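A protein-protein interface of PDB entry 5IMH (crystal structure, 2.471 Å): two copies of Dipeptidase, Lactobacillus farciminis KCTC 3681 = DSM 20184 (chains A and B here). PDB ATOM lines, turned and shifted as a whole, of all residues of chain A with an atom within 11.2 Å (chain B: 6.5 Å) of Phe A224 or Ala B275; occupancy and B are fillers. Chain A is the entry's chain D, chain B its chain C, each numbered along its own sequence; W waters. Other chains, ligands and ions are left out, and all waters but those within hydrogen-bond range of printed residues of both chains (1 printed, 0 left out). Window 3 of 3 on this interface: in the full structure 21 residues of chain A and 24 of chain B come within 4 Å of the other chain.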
ATOM      1  N   LYS A 212     -16.068 -15.498   0.816  1.00  0.00           N
ATOM      2  CA  LYS A 212     -17.274 -16.185   1.280  1.00  0.00           C
ATOM      3  C   LYS A 212     -17.375 -17.614   0.713  1.00  0.00           C
ATOM      4  O   LYS A 212     -17.647 -18.574   1.450  1.00  0.00           O
ATOM      5  CB  LYS A 212     -18.522 -15.369   0.915  1.00  0.00           C
ATOM      6  CG  LYS A 212     -19.841 -16.037   1.296  1.00  0.00           C
ATOM      7  CD  LYS A 212     -20.963 -15.008   1.439  1.00  0.00           C
ATOM      8  CE  LYS A 212     -22.321 -15.682   1.588  1.00  0.00           C
ATOM      9  NZ  LYS A 212     -22.204 -17.107   1.962  1.00  0.00           N
ATOM     10  N   ILE A 215     -14.950 -20.006   2.361  1.00  0.00           N
ATOM     11  CA  ILE A 215     -15.397 -20.494   3.656  1.00  0.00           C
ATOM     12  C   ILE A 215     -16.498 -21.541   3.489  1.00  0.00           C
ATOM     13  O   ILE A 215     -16.322 -22.685   3.894  1.00  0.00           O
ATOM     14  CB  ILE A 215     -15.929 -19.349   4.554  1.00  0.00           C
ATOM     15  CG1 ILE A 215     -14.866 -18.283   4.778  1.00  0.00           C
ATOM     16  CG2 ILE A 215     -16.452 -19.909   5.877  1.00  0.00           C
ATOM     17  CD1 ILE A 215     -15.438 -16.980   5.276  1.00  0.00           C
ATOM     18  N   ASP A 216     -17.590 -21.157   2.830  1.00  0.00           N
ATOM     19  CA  ASP A 216     -18.772 -22.016   2.679  1.00  0.00           C
ATOM     20  C   ASP A 216     -18.477 -23.372   2.025  1.00  0.00           C
ATOM     21  O   ASP A 216     -19.069 -24.385   2.396  1.00  0.00           O
ATOM     22  CB  ASP A 216     -19.850 -21.294   1.865  1.00  0.00           C
ATOM     23  CG  ASP A 216     -20.401 -20.093   2.580  1.00  0.00           C
ATOM     24  OD1 ASP A 216     -20.232 -20.000   3.816  1.00  0.00           O
ATOM     25  OD2 ASP A 216     -21.010 -19.237   1.906  1.00  0.00           O
ATOM     26  N   ASN A 219     -15.931 -26.075   4.697  1.00  0.00           N
ATOM     27  CA  ASN A 219     -16.177 -26.325   6.133  1.00  0.00           C
ATOM     28  C   ASN A 219     -15.228 -25.548   7.024  1.00  0.00           C
ATOM     29  O   ASN A 219     -14.627 -26.129   7.935  1.00  0.00           O
ATOM     30  CB  ASN A 219     -16.040 -27.805   6.489  1.00  0.00           C
ATOM     31  CG  ASN A 219     -17.008 -28.673   5.744  1.00  0.00           C
ATOM     32  OD1 ASN A 219     -18.214 -28.583   5.946  1.00  0.00           O
ATOM     33  ND2 ASN A 219     -16.483 -29.564   4.912  1.00  0.00           N
ATOM     34  N   LEU A 220     -15.018 -24.272   6.710  1.00  0.00           N
ATOM     35  CA  LEU A 220     -14.131 -23.434   7.502  1.00  0.00           C
ATOM     36  C   LEU A 220     -14.855 -22.756   8.648  1.00  0.00           C
ATOM     37  O   LEU A 220     -14.223 -22.305   9.606  1.00  0.00           O
ATOM     38  CB  LEU A 220     -13.475 -22.367   6.632  1.00  0.00           C
ATOM     39  CG  LEU A 220     -12.357 -22.859   5.722  1.00  0.00           C
ATOM     40  CD1 LEU A 220     -11.683 -21.685   5.018  1.00  0.00           C
ATOM     41  CD2 LEU A 220     -11.371 -23.684   6.519  1.00  0.00           C
ATOM     42  N   ASN A 221     -16.172 -22.647   8.527  1.00  0.00           N
ATOM     43  CA  ASN A 221     -16.978 -21.885   9.480  1.00  0.00           C
ATOM     44  C   ASN A 221     -17.351 -22.779  10.666  1.00  0.00           C
ATOM     45  O   ASN A 221     -17.929 -23.857  10.484  1.00  0.00           O
ATOM     46  CB  ASN A 221     -18.239 -21.295   8.798  1.00  0.00           C
ATOM     47  CG  ASN A 221     -18.827 -20.100   9.557  1.00  0.00           C
ATOM     48  OD1 ASN A 221     -18.630 -19.966  10.769  1.00  0.00           O
ATOM     49  ND2 ASN A 221     -19.551 -19.225   8.844  1.00  0.00           N
ATOM     50  N   PRO A 222     -16.908 -22.393  11.866  1.00  0.00           N
ATOM     51  CA  PRO A 222     -17.229 -23.130  13.088  1.00  0.00           C
ATOM     52  C   PRO A 222     -18.566 -22.662  13.736  1.00  0.00           C
ATOM     53  O   PRO A 222     -19.122 -23.349  14.601  1.00  0.00           O
ATOM     54  CB  PRO A 222     -16.035 -22.806  13.992  1.00  0.00           C
ATOM     55  CG  PRO A 222     -15.680 -21.414  13.621  1.00  0.00           C
ATOM     56  CD  PRO A 222     -15.950 -21.305  12.125  1.00  0.00           C
ATOM     57  N   ASP A 223     -19.080 -21.512  13.311  1.00  0.00           N
ATOM     58  CA  ASP A 223     -20.226 -20.930  13.990  1.00  0.00           C
ATOM     59  C   ASP A 223     -21.517 -21.360  13.309  1.00  0.00           C
ATOM     60  O   ASP A 223     -21.534 -21.589  12.103  1.00  0.00           O
ATOM     61  CB  ASP A 223     -20.104 -19.410  14.036  1.00  0.00           C
ATOM     62  CG  ASP A 223     -19.025 -18.952  14.997  1.00  0.00           C
ATOM     63  OD1 ASP A 223     -19.089 -19.360  16.160  1.00  0.00           O
ATOM     64  OD2 ASP A 223     -18.088 -18.222  14.608  1.00  0.00           O
ATOM     65  N   PHE A 224     -22.579 -21.504  14.100  1.00  0.00           N
ATOM     66  CA  PHE A 224     -23.872 -21.942  13.588  1.00  0.00           C
ATOM     67  C   PHE A 224     -24.460 -20.884  12.687  1.00  0.00           C
ATOM     68  O   PHE A 224     -25.083 -21.210  11.686  1.00  0.00           O
ATOM     69  CB  PHE A 224     -24.842 -22.277  14.727  1.00  0.00           C
ATOM     70  CG  PHE A 224     -24.311 -23.315  15.668  1.00  0.00           C
ATOM     71  CD1 PHE A 224     -23.804 -24.506  15.176  1.00  0.00           C
ATOM     72  CD2 PHE A 224     -24.282 -23.086  17.044  1.00  0.00           C
ATOM     73  CE1 PHE A 224     -23.282 -25.462  16.040  1.00  0.00           C
ATOM     74  CE2 PHE A 224     -23.774 -24.038  17.903  1.00  0.00           C
ATOM     75  CZ  PHE A 224     -23.267 -25.223  17.407  1.00  0.00           C
ATOM     76  N   GLU A 225     -24.256 -19.620  13.035  1.00  0.00           N
ATOM     77  CA  GLU A 225     -24.743 -18.525  12.205  1.00  0.00           C
ATOM     78  C   GLU A 225     -23.699 -17.478  11.888  1.00  0.00           C
ATOM     79  O   GLU A 225     -22.759 -17.253  12.673  1.00  0.00           O
ATOM     80  CB  GLU A 225     -25.917 -17.837  12.879  1.00  0.00           C
ATOM     81  CG  GLU A 225     -27.044 -18.787  13.169  1.00  0.00           C
ATOM     82  CD  GLU A 225     -28.245 -18.079  13.726  1.00  0.00           C
ATOM     83  OE1 GLU A 225     -28.065 -16.987  14.319  1.00  0.00           O
ATOM     84  OE2 GLU A 225     -29.358 -18.627  13.583  1.00  0.00           O
ATOM     85  N   ASN A 226     -23.875 -16.855  10.720  1.00  0.00           N
ATOM     86  CA  ASN A 226     -23.137 -15.655  10.336  1.00  0.00           C
ATOM     87  C   ASN A 226     -21.641 -15.908  10.227  1.00  0.00           C
ATOM     88  O   ASN A 226     -21.198 -17.058  10.273  1.00  0.00           O
ATOM     89  CB  ASN A 226     -23.415 -14.529  11.329  1.00  0.00           C
ATOM     90  CG  ASN A 226     -24.899 -14.242  11.467  1.00  0.00           C
ATOM     91  OD1 ASN A 226     -25.605 -14.108  10.470  1.00  0.00           O
ATOM     92  ND2 ASN A 226     -25.379 -14.146  12.705  1.00  0.00           N
ATOM     93  N   TYR A 227     -20.868 -14.834  10.068  1.00  0.00           N
ATOM     94  CA  TYR A 227     -19.432 -14.963   9.837  1.00  0.00           C
ATOM     95  C   TYR A 227     -18.626 -14.079  10.779  1.00  0.00           C
ATOM     96  O   TYR A 227     -18.758 -12.847  10.803  1.00  0.00           O
ATOM     97  CB  TYR A 227     -19.079 -14.625   8.382  1.00  0.00           C
ATOM     98  CG  TYR A 227     -19.717 -15.525   7.350  1.00  0.00           C
ATOM     99  CD1 TYR A 227     -21.000 -15.274   6.879  1.00  0.00           C
ATOM    100  CD2 TYR A 227     -19.032 -16.612   6.827  1.00  0.00           C
ATOM    101  CE1 TYR A 227     -21.587 -16.093   5.926  1.00  0.00           C
ATOM    102  CE2 TYR A 227     -19.607 -17.436   5.865  1.00  0.00           C
ATOM    103  CZ  TYR A 227     -20.883 -17.171   5.423  1.00  0.00           C
ATOM    104  OH  TYR A 227     -21.474 -17.984   4.482  1.00  0.00           O
ATOM    105  N   ASN A 228     -17.775 -14.739  11.545  1.00  0.00           N
ATOM    106  CA  ASN A 228     -16.822 -14.089  12.410  1.00  0.00           C
ATOM    107  C   ASN A 228     -15.458 -14.452  11.873  1.00  0.00           C
ATOM    108  O   ASN A 228     -15.044 -15.609  11.989  1.00  0.00           O
ATOM    109  CB  ASN A 228     -17.007 -14.566  13.856  1.00  0.00           C
ATOM    110  CG  ASN A 228     -16.057 -13.892  14.832  1.00  0.00           C
ATOM    111  OD1 ASN A 228     -14.861 -13.724  14.562  1.00  0.00           O
ATOM    112  ND2 ASN A 228     -16.597 -13.482  15.972  1.00  0.00           N
ATOM    113  N   HIS A 231     -12.810 -16.114  14.162  1.00  0.00           N
ATOM    114  CA  HIS A 231     -13.257 -17.464  14.483  1.00  0.00           C
ATOM    115  C   HIS A 231     -12.910 -18.418  13.362  1.00  0.00           C
ATOM    116  O   HIS A 231     -12.486 -19.549  13.598  1.00  0.00           O
ATOM    117  CB  HIS A 231     -14.763 -17.507  14.716  1.00  0.00           C
ATOM    118  CG  HIS A 231     -15.196 -16.956  16.032  1.00  0.00           C
ATOM    119  ND1 HIS A 231     -16.511 -16.980  16.448  1.00  0.00           N
ATOM    120  CD2 HIS A 231     -14.491 -16.377  17.033  1.00  0.00           C
ATOM    121  CE1 HIS A 231     -16.598 -16.425  17.643  1.00  0.00           C
ATOM    122  NE2 HIS A 231     -15.385 -16.058  18.023  1.00  0.00           N
ATOM    123  N   ILE A 232     -13.124 -17.947  12.135  1.00  0.00           N
ATOM    124  CA  ILE A 232     -12.987 -18.758  10.933  1.00  0.00           C
ATOM    125  C   ILE A 232     -11.529 -18.942  10.548  1.00  0.00           C
ATOM    126  O   ILE A 232     -11.092 -20.068  10.332  1.00  0.00           O
ATOM    127  CB  ILE A 232     -13.757 -18.108   9.744  1.00  0.00           C
ATOM    128  CG1 ILE A 232     -15.251 -18.033  10.030  1.00  0.00           C
ATOM    129  CG2 ILE A 232     -13.545 -18.866   8.449  1.00  0.00           C
ATOM    130  CD1 ILE A 232     -15.979 -17.086   9.119  1.00  0.00           C
ATOM    131  N   LYS B  17     -23.266 -33.881  13.143  1.00  0.00           N
ATOM    132  CA  LYS B  17     -23.660 -32.481  12.957  1.00  0.00           C
ATOM    133  C   LYS B  17     -22.967 -31.542  13.941  1.00  0.00           C
ATOM    134  O   LYS B  17     -23.161 -30.321  13.881  1.00  0.00           O
ATOM    135  CB  LYS B  17     -25.165 -32.303  13.078  1.00  0.00           C
ATOM    136  CG  LYS B  17     -25.973 -33.021  12.008  1.00  0.00           C
ATOM    137  CD  LYS B  17     -27.422 -32.659  12.154  1.00  0.00           C
ATOM    138  CE  LYS B  17     -28.286 -33.397  11.162  1.00  0.00           C
ATOM    139  NZ  LYS B  17     -29.670 -33.445  11.671  1.00  0.00           N
ATOM    140  N   ALA B  18     -22.193 -32.114  14.865  1.00  0.00           N
ATOM    141  CA  ALA B  18     -21.494 -31.331  15.886  1.00  0.00           C
ATOM    142  C   ALA B  18     -20.055 -30.951  15.470  1.00  0.00           C
ATOM    143  O   ALA B  18     -19.433 -30.085  16.073  1.00  0.00           O
ATOM    144  CB  ALA B  18     -21.489 -32.082  17.210  1.00  0.00           C
ATOM    145  N   ASP B 184     -25.889 -33.638  17.051  1.00  0.00           N
ATOM    146  CA  ASP B 184     -25.420 -32.296  17.358  1.00  0.00           C
ATOM    147  C   ASP B 184     -24.717 -32.218  18.716  1.00  0.00           C
ATOM    148  O   ASP B 184     -24.524 -31.134  19.264  1.00  0.00           O
ATOM    149  CB  ASP B 184     -26.589 -31.306  17.307  1.00  0.00           C
ATOM    150  CG  ASP B 184     -27.656 -31.575  18.364  1.00  0.00           C
ATOM    151  OD1 ASP B 184     -27.670 -32.661  18.986  1.00  0.00           O
ATOM    152  OD2 ASP B 184     -28.508 -30.680  18.562  1.00  0.00           O
ATOM    153  N   ALA B 185     -24.357 -33.367  19.274  1.00  0.00           N
ATOM    154  CA  ALA B 185     -23.792 -33.366  20.618  1.00  0.00           C
ATOM    155  C   ALA B 185     -22.339 -33.847  20.653  1.00  0.00           C
ATOM    156  O   ALA B 185     -21.792 -34.370  19.659  1.00  0.00           O
ATOM    157  CB  ALA B 185     -24.626 -34.205  21.539  1.00  0.00           C
ATOM    158  N   TYR B 186     -21.737 -33.689  21.825  1.00  0.00           N
ATOM    159  CA  TYR B 186     -20.407 -34.207  22.066  1.00  0.00           C
ATOM    160  C   TYR B 186     -20.341 -34.772  23.448  1.00  0.00           C
ATOM    161  O   TYR B 186     -21.182 -34.471  24.290  1.00  0.00           O
ATOM    162  CB  TYR B 186     -19.338 -33.122  21.887  1.00  0.00           C
ATOM    163  CG  TYR B 186     -19.295 -32.116  23.017  1.00  0.00           C
ATOM    164  CD1 TYR B 186     -20.096 -30.980  22.991  1.00  0.00           C
ATOM    165  CD2 TYR B 186     -18.450 -32.303  24.119  1.00  0.00           C
ATOM    166  CE1 TYR B 186     -20.059 -30.060  24.023  1.00  0.00           C
ATOM    167  CE2 TYR B 186     -18.416 -31.390  25.158  1.00  0.00           C
ATOM    168  CZ  TYR B 186     -19.226 -30.273  25.103  1.00  0.00           C
ATOM    169  OH  TYR B 186     -19.190 -29.352  26.119  1.00  0.00           O
ATOM    170  N   PHE B 255     -15.829 -26.345  25.443  1.00  0.00           N
ATOM    171  CA  PHE B 255     -16.834 -26.412  24.384  1.00  0.00           C
ATOM    172  C   PHE B 255     -18.153 -25.741  24.783  1.00  0.00           C
ATOM    173  O   PHE B 255     -18.864 -25.185  23.928  1.00  0.00           O
ATOM    174  CB  PHE B 255     -17.088 -27.859  24.010  1.00  0.00           C
ATOM    175  CG  PHE B 255     -15.949 -28.510  23.284  1.00  0.00           C
ATOM    176  CD1 PHE B 255     -15.481 -27.989  22.072  1.00  0.00           C
ATOM    177  CD2 PHE B 255     -15.342 -29.644  23.809  1.00  0.00           C
ATOM    178  CE1 PHE B 255     -14.457 -28.600  21.394  1.00  0.00           C
ATOM    179  CE2 PHE B 255     -14.295 -30.266  23.146  1.00  0.00           C
ATOM    180  CZ  PHE B 255     -13.848 -29.748  21.930  1.00  0.00           C
ATOM    181  N   SER B 256     -18.490 -25.790  26.075  1.00  0.00           N
ATOM    182  CA  SER B 256     -19.743 -25.189  26.548  1.00  0.00           C
ATOM    183  C   SER B 256     -19.532 -24.244  27.721  1.00  0.00           C
ATOM    184  O   SER B 256     -20.051 -24.501  28.820  1.00  0.00           O
ATOM    185  CB  SER B 256     -20.734 -26.281  26.967  1.00  0.00           C
ATOM    186  OG  SER B 256     -20.907 -27.248  25.954  1.00  0.00           O
ATOM    187  N   PRO B 257     -18.795 -23.138  27.501  1.00  0.00           N
ATOM    188  CA  PRO B 257     -18.439 -22.262  28.629  1.00  0.00           C
ATOM    189  C   PRO B 257     -19.652 -21.687  29.363  1.00  0.00           C
ATOM    190  O   PRO B 257     -19.561 -21.499  30.581  1.00  0.00           O
ATOM    191  CB  PRO B 257     -17.600 -21.137  27.966  1.00  0.00           C
ATOM    192  CG  PRO B 257     -17.955 -21.196  26.490  1.00  0.00           C
ATOM    193  CD  PRO B 257     -18.231 -22.656  26.222  1.00  0.00           C
ATOM    194  N   ASP B 259     -22.719 -23.110  29.694  1.00  0.00           N
ATOM    195  CA  ASP B 259     -23.598 -24.111  30.310  1.00  0.00           C
ATOM    196  C   ASP B 259     -22.879 -24.854  31.424  1.00  0.00           C
ATOM    197  O   ASP B 259     -23.382 -25.825  31.960  1.00  0.00           O
ATOM    198  CB  ASP B 259     -24.082 -25.165  29.311  1.00  0.00           C
ATOM    199  CG  ASP B 259     -24.704 -24.573  28.061  1.00  0.00           C
ATOM    200  OD1 ASP B 259     -25.241 -23.437  28.101  1.00  0.00           O
ATOM    201  OD2 ASP B 259     -24.724 -25.317  27.050  1.00  0.00           O
ATOM    202  N   CYS B 273     -23.659 -33.350  25.735  1.00  0.00           N
ATOM    203  CA  CYS B 273     -23.512 -31.905  25.782  1.00  0.00           C
ATOM    204  C   CYS B 273     -23.723 -31.236  24.433  1.00  0.00           C
ATOM    205  O   CYS B 273     -23.693 -31.877  23.382  1.00  0.00           O
ATOM    206  CB  CYS B 273     -22.125 -31.512  26.313  1.00  0.00           C
ATOM    207  SG  CYS B 273     -21.769 -31.946  28.015  1.00  0.00           S
ATOM    208  N   HIS B 274     -23.915 -29.925  24.469  1.00  0.00           N
ATOM    209  CA  HIS B 274     -24.027 -29.160  23.234  1.00  0.00           C
ATOM    210  C   HIS B 274     -23.094 -27.997  23.310  1.00  0.00           C
ATOM    211  O   HIS B 274     -23.227 -27.135  24.183  1.00  0.00           O
ATOM    212  CB  HIS B 274     -25.471 -28.714  22.995  1.00  0.00           C
ATOM    213  CG  HIS B 274     -26.413 -29.867  22.861  1.00  0.00           C
ATOM    214  ND1 HIS B 274     -26.896 -30.565  23.950  1.00  0.00           N
ATOM    215  CD2 HIS B 274     -26.906 -30.490  21.765  1.00  0.00           C
ATOM    216  CE1 HIS B 274     -27.665 -31.551  23.529  1.00  0.00           C
ATOM    217  NE2 HIS B 274     -27.685 -31.529  22.208  1.00  0.00           N
ATOM    218  N   ALA B 275     -22.134 -27.987  22.391  1.00  0.00           N
ATOM    219  CA  ALA B 275     -21.115 -26.942  22.332  1.00  0.00           C
ATOM    220  C   ALA B 275     -21.706 -25.676  21.734  1.00  0.00           C
ATOM    221  O   ALA B 275     -22.759 -25.710  21.083  1.00  0.00           O
ATOM    222  CB  ALA B 275     -19.934 -27.409  21.529  1.00  0.00           C
ATOM    223  N   ASN B 276     -21.028 -24.555  21.949  1.00  0.00           N
ATOM    224  CA  ASN B 276     -21.499 -23.281  21.414  1.00  0.00           C
ATOM    225  C   ASN B 276     -21.000 -23.037  19.996  1.00  0.00           C
ATOM    226  O   ASN B 276     -21.162 -21.946  19.478  1.00  0.00           O
ATOM    227  CB  ASN B 276     -21.067 -22.115  22.313  1.00  0.00           C
ATOM    228  CG  ASN B 276     -19.559 -21.970  22.412  1.00  0.00           C
ATOM    229  OD1 ASN B 276     -18.793 -22.685  21.759  1.00  0.00           O
ATOM    230  ND2 ASN B 276     -19.123 -21.021  23.220  1.00  0.00           N
ATOM    231  N   ARG B 277     -20.397 -24.064  19.393  1.00  0.00           N
ATOM    232  CA  ARG B 277     -19.770 -23.973  18.077  1.00  0.00           C
ATOM    233  C   ARG B 277     -19.484 -25.379  17.556  1.00  0.00           C
ATOM    234  O   ARG B 277     -19.631 -26.348  18.273  1.00  0.00           O
ATOM    235  CB  ARG B 277     -18.479 -23.143  18.140  1.00  0.00           C
ATOM    236  CG  ARG B 277     -17.342 -23.775  18.979  1.00  0.00           C
ATOM    237  CD  ARG B 277     -16.309 -22.729  19.442  1.00  0.00           C
ATOM    238  NE  ARG B 277     -15.172 -23.321  20.135  1.00  0.00           N
ATOM    239  CZ  ARG B 277     -15.127 -23.580  21.447  1.00  0.00           C
ATOM    240  NH1 ARG B 277     -16.169 -23.323  22.228  1.00  0.00           N
ATOM    241  NH2 ARG B 277     -14.040 -24.121  21.982  1.00  0.00           N
ATOM    242  N   LYS B 278     -19.137 -25.499  16.289  1.00  0.00           N
ATOM    243  CA  LYS B 278     -18.769 -26.793  15.746  1.00  0.00           C
ATOM    244  C   LYS B 278     -17.326 -27.112  16.119  1.00  0.00           C
ATOM    245  O   LYS B 278     -16.486 -26.210  16.250  1.00  0.00           O
ATOM    246  CB  LYS B 278     -18.940 -26.812  14.238  1.00  0.00           C
ATOM    247  CG  LYS B 278     -20.351 -26.456  13.740  1.00  0.00           C
ATOM    248  CD  LYS B 278     -20.328 -26.448  12.217  1.00  0.00           C
ATOM    249  CE  LYS B 278     -21.654 -26.139  11.596  1.00  0.00           C
ATOM    250  NZ  LYS B 278     -21.453 -26.227  10.116  1.00  0.00           N
ATOM    251  N   ILE B 279     -17.042 -28.402  16.262  1.00  0.00           N
ATOM    252  CA  ILE B 279     -15.777 -28.869  16.796  1.00  0.00           C
ATOM    253  C   ILE B 279     -14.820 -29.351  15.721  1.00  0.00           C
ATOM    254  O   ILE B 279     -15.208 -30.119  14.846  1.00  0.00           O
ATOM    255  CB  ILE B 279     -16.019 -30.011  17.788  1.00  0.00           C
ATOM    256  CG1 ILE B 279     -16.992 -29.540  18.886  1.00  0.00           C
ATOM    257  CG2 ILE B 279     -14.704 -30.537  18.322  1.00  0.00           C
ATOM    258  CD1 ILE B 279     -17.389 -30.621  19.899  1.00  0.00           C
HETATM  259  O   HOH W   1     -18.869 -25.710   9.200  1.00  0.00           O
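Asn A221 touches Lys B278. Arg B277 touches Pro A222. CE2 of Phe A224 touches O of Ala B275, 3.7 Å away. Asn B276 touches Phe A224. CZ of Phe A224 touches N of Arg B277 (3.7 Å). Lys B278 touches Phe A224 (CG to CE1, 3.9 Å).
No position is printed for both chains.
The backbone NH (N) of Asn B276 lies within hydrogen-bond range of the backbone carbonyl oxygen (O) of Phe B255, at 3.0 Å. The side-chain amide oxygen (OD1) of Asn B276 sits at hydrogen-bond distance from the guanidinium group (NH1) of Arg B277, 2.7 Å away. The backbone NH (N) of Asp A223 lies within hydrogen-bond range of the side-chain amide oxygen (OD1) of Asn A221, 3.0 Å away. ND2 of Asn A221 lies within hydrogen-bond range of O of Asn A226 (3.1 Å).
Water W1 lies within hydrogen-bond range of the backbone carbonyl oxygen (O) of Asn A221 (2.4 Å) and the side-chain amino group (NZ) of Lys B278 (2.8 Å).
Of the printed residues of chain B, Asn A221 touches Lys B278. Printed residues of chain B within 4 Å of Pro A222: Arg B277 (3.6 Å) and Lys B278 (2.7 Å). Phe A224 touches just these residues of chain B: Ala B275 (3.7 Å), Asn B276 (3.6 Å), Arg B277 (3.7 Å) and Lys B278 (3.9 Å). No residue of chain A comes within 4 Å of Ala B18. Ala B185 touches none of the printed residues of chain A. No residue of chain A comes within 4 Å of Tyr B186. No residue of chain A comes within 4 Å of Cys B273. No residue of chain A comes within 4 Å of His B274. Ala B275 touches just one residue of chain A: Phe A224 (3.7 Å). Asn B276 touches just one residue of chain A: Phe A224. Of chain A, only Pro A222 and Phe A224 come within 4 Å of Arg B277. Lys B278 touches just these residues of chain A: Asn A221 (3.9 Å), Pro A222 (2.7 Å) and Phe A224 (3.9 Å). The nearest residue of chain A that does not touch Ala B275 is Pro A222 (7.8 Å).
O of Pro A222 sits at hydrogen-bond distance from N of Lys B278, 2.7 Å away.
Of the 15 printed residues of chain A, 3 touch a printed residue of chain B. Hydrophobic or aromatic side chains of chain A that line the printed part of chain B: Phe A224. Among the printed residues, 7 pairs touch across the chains. Among the printed residues, no Asp or Glu carboxylate lies within 4 Å of a Lys or Arg side-chain nitrogen of the other chain.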
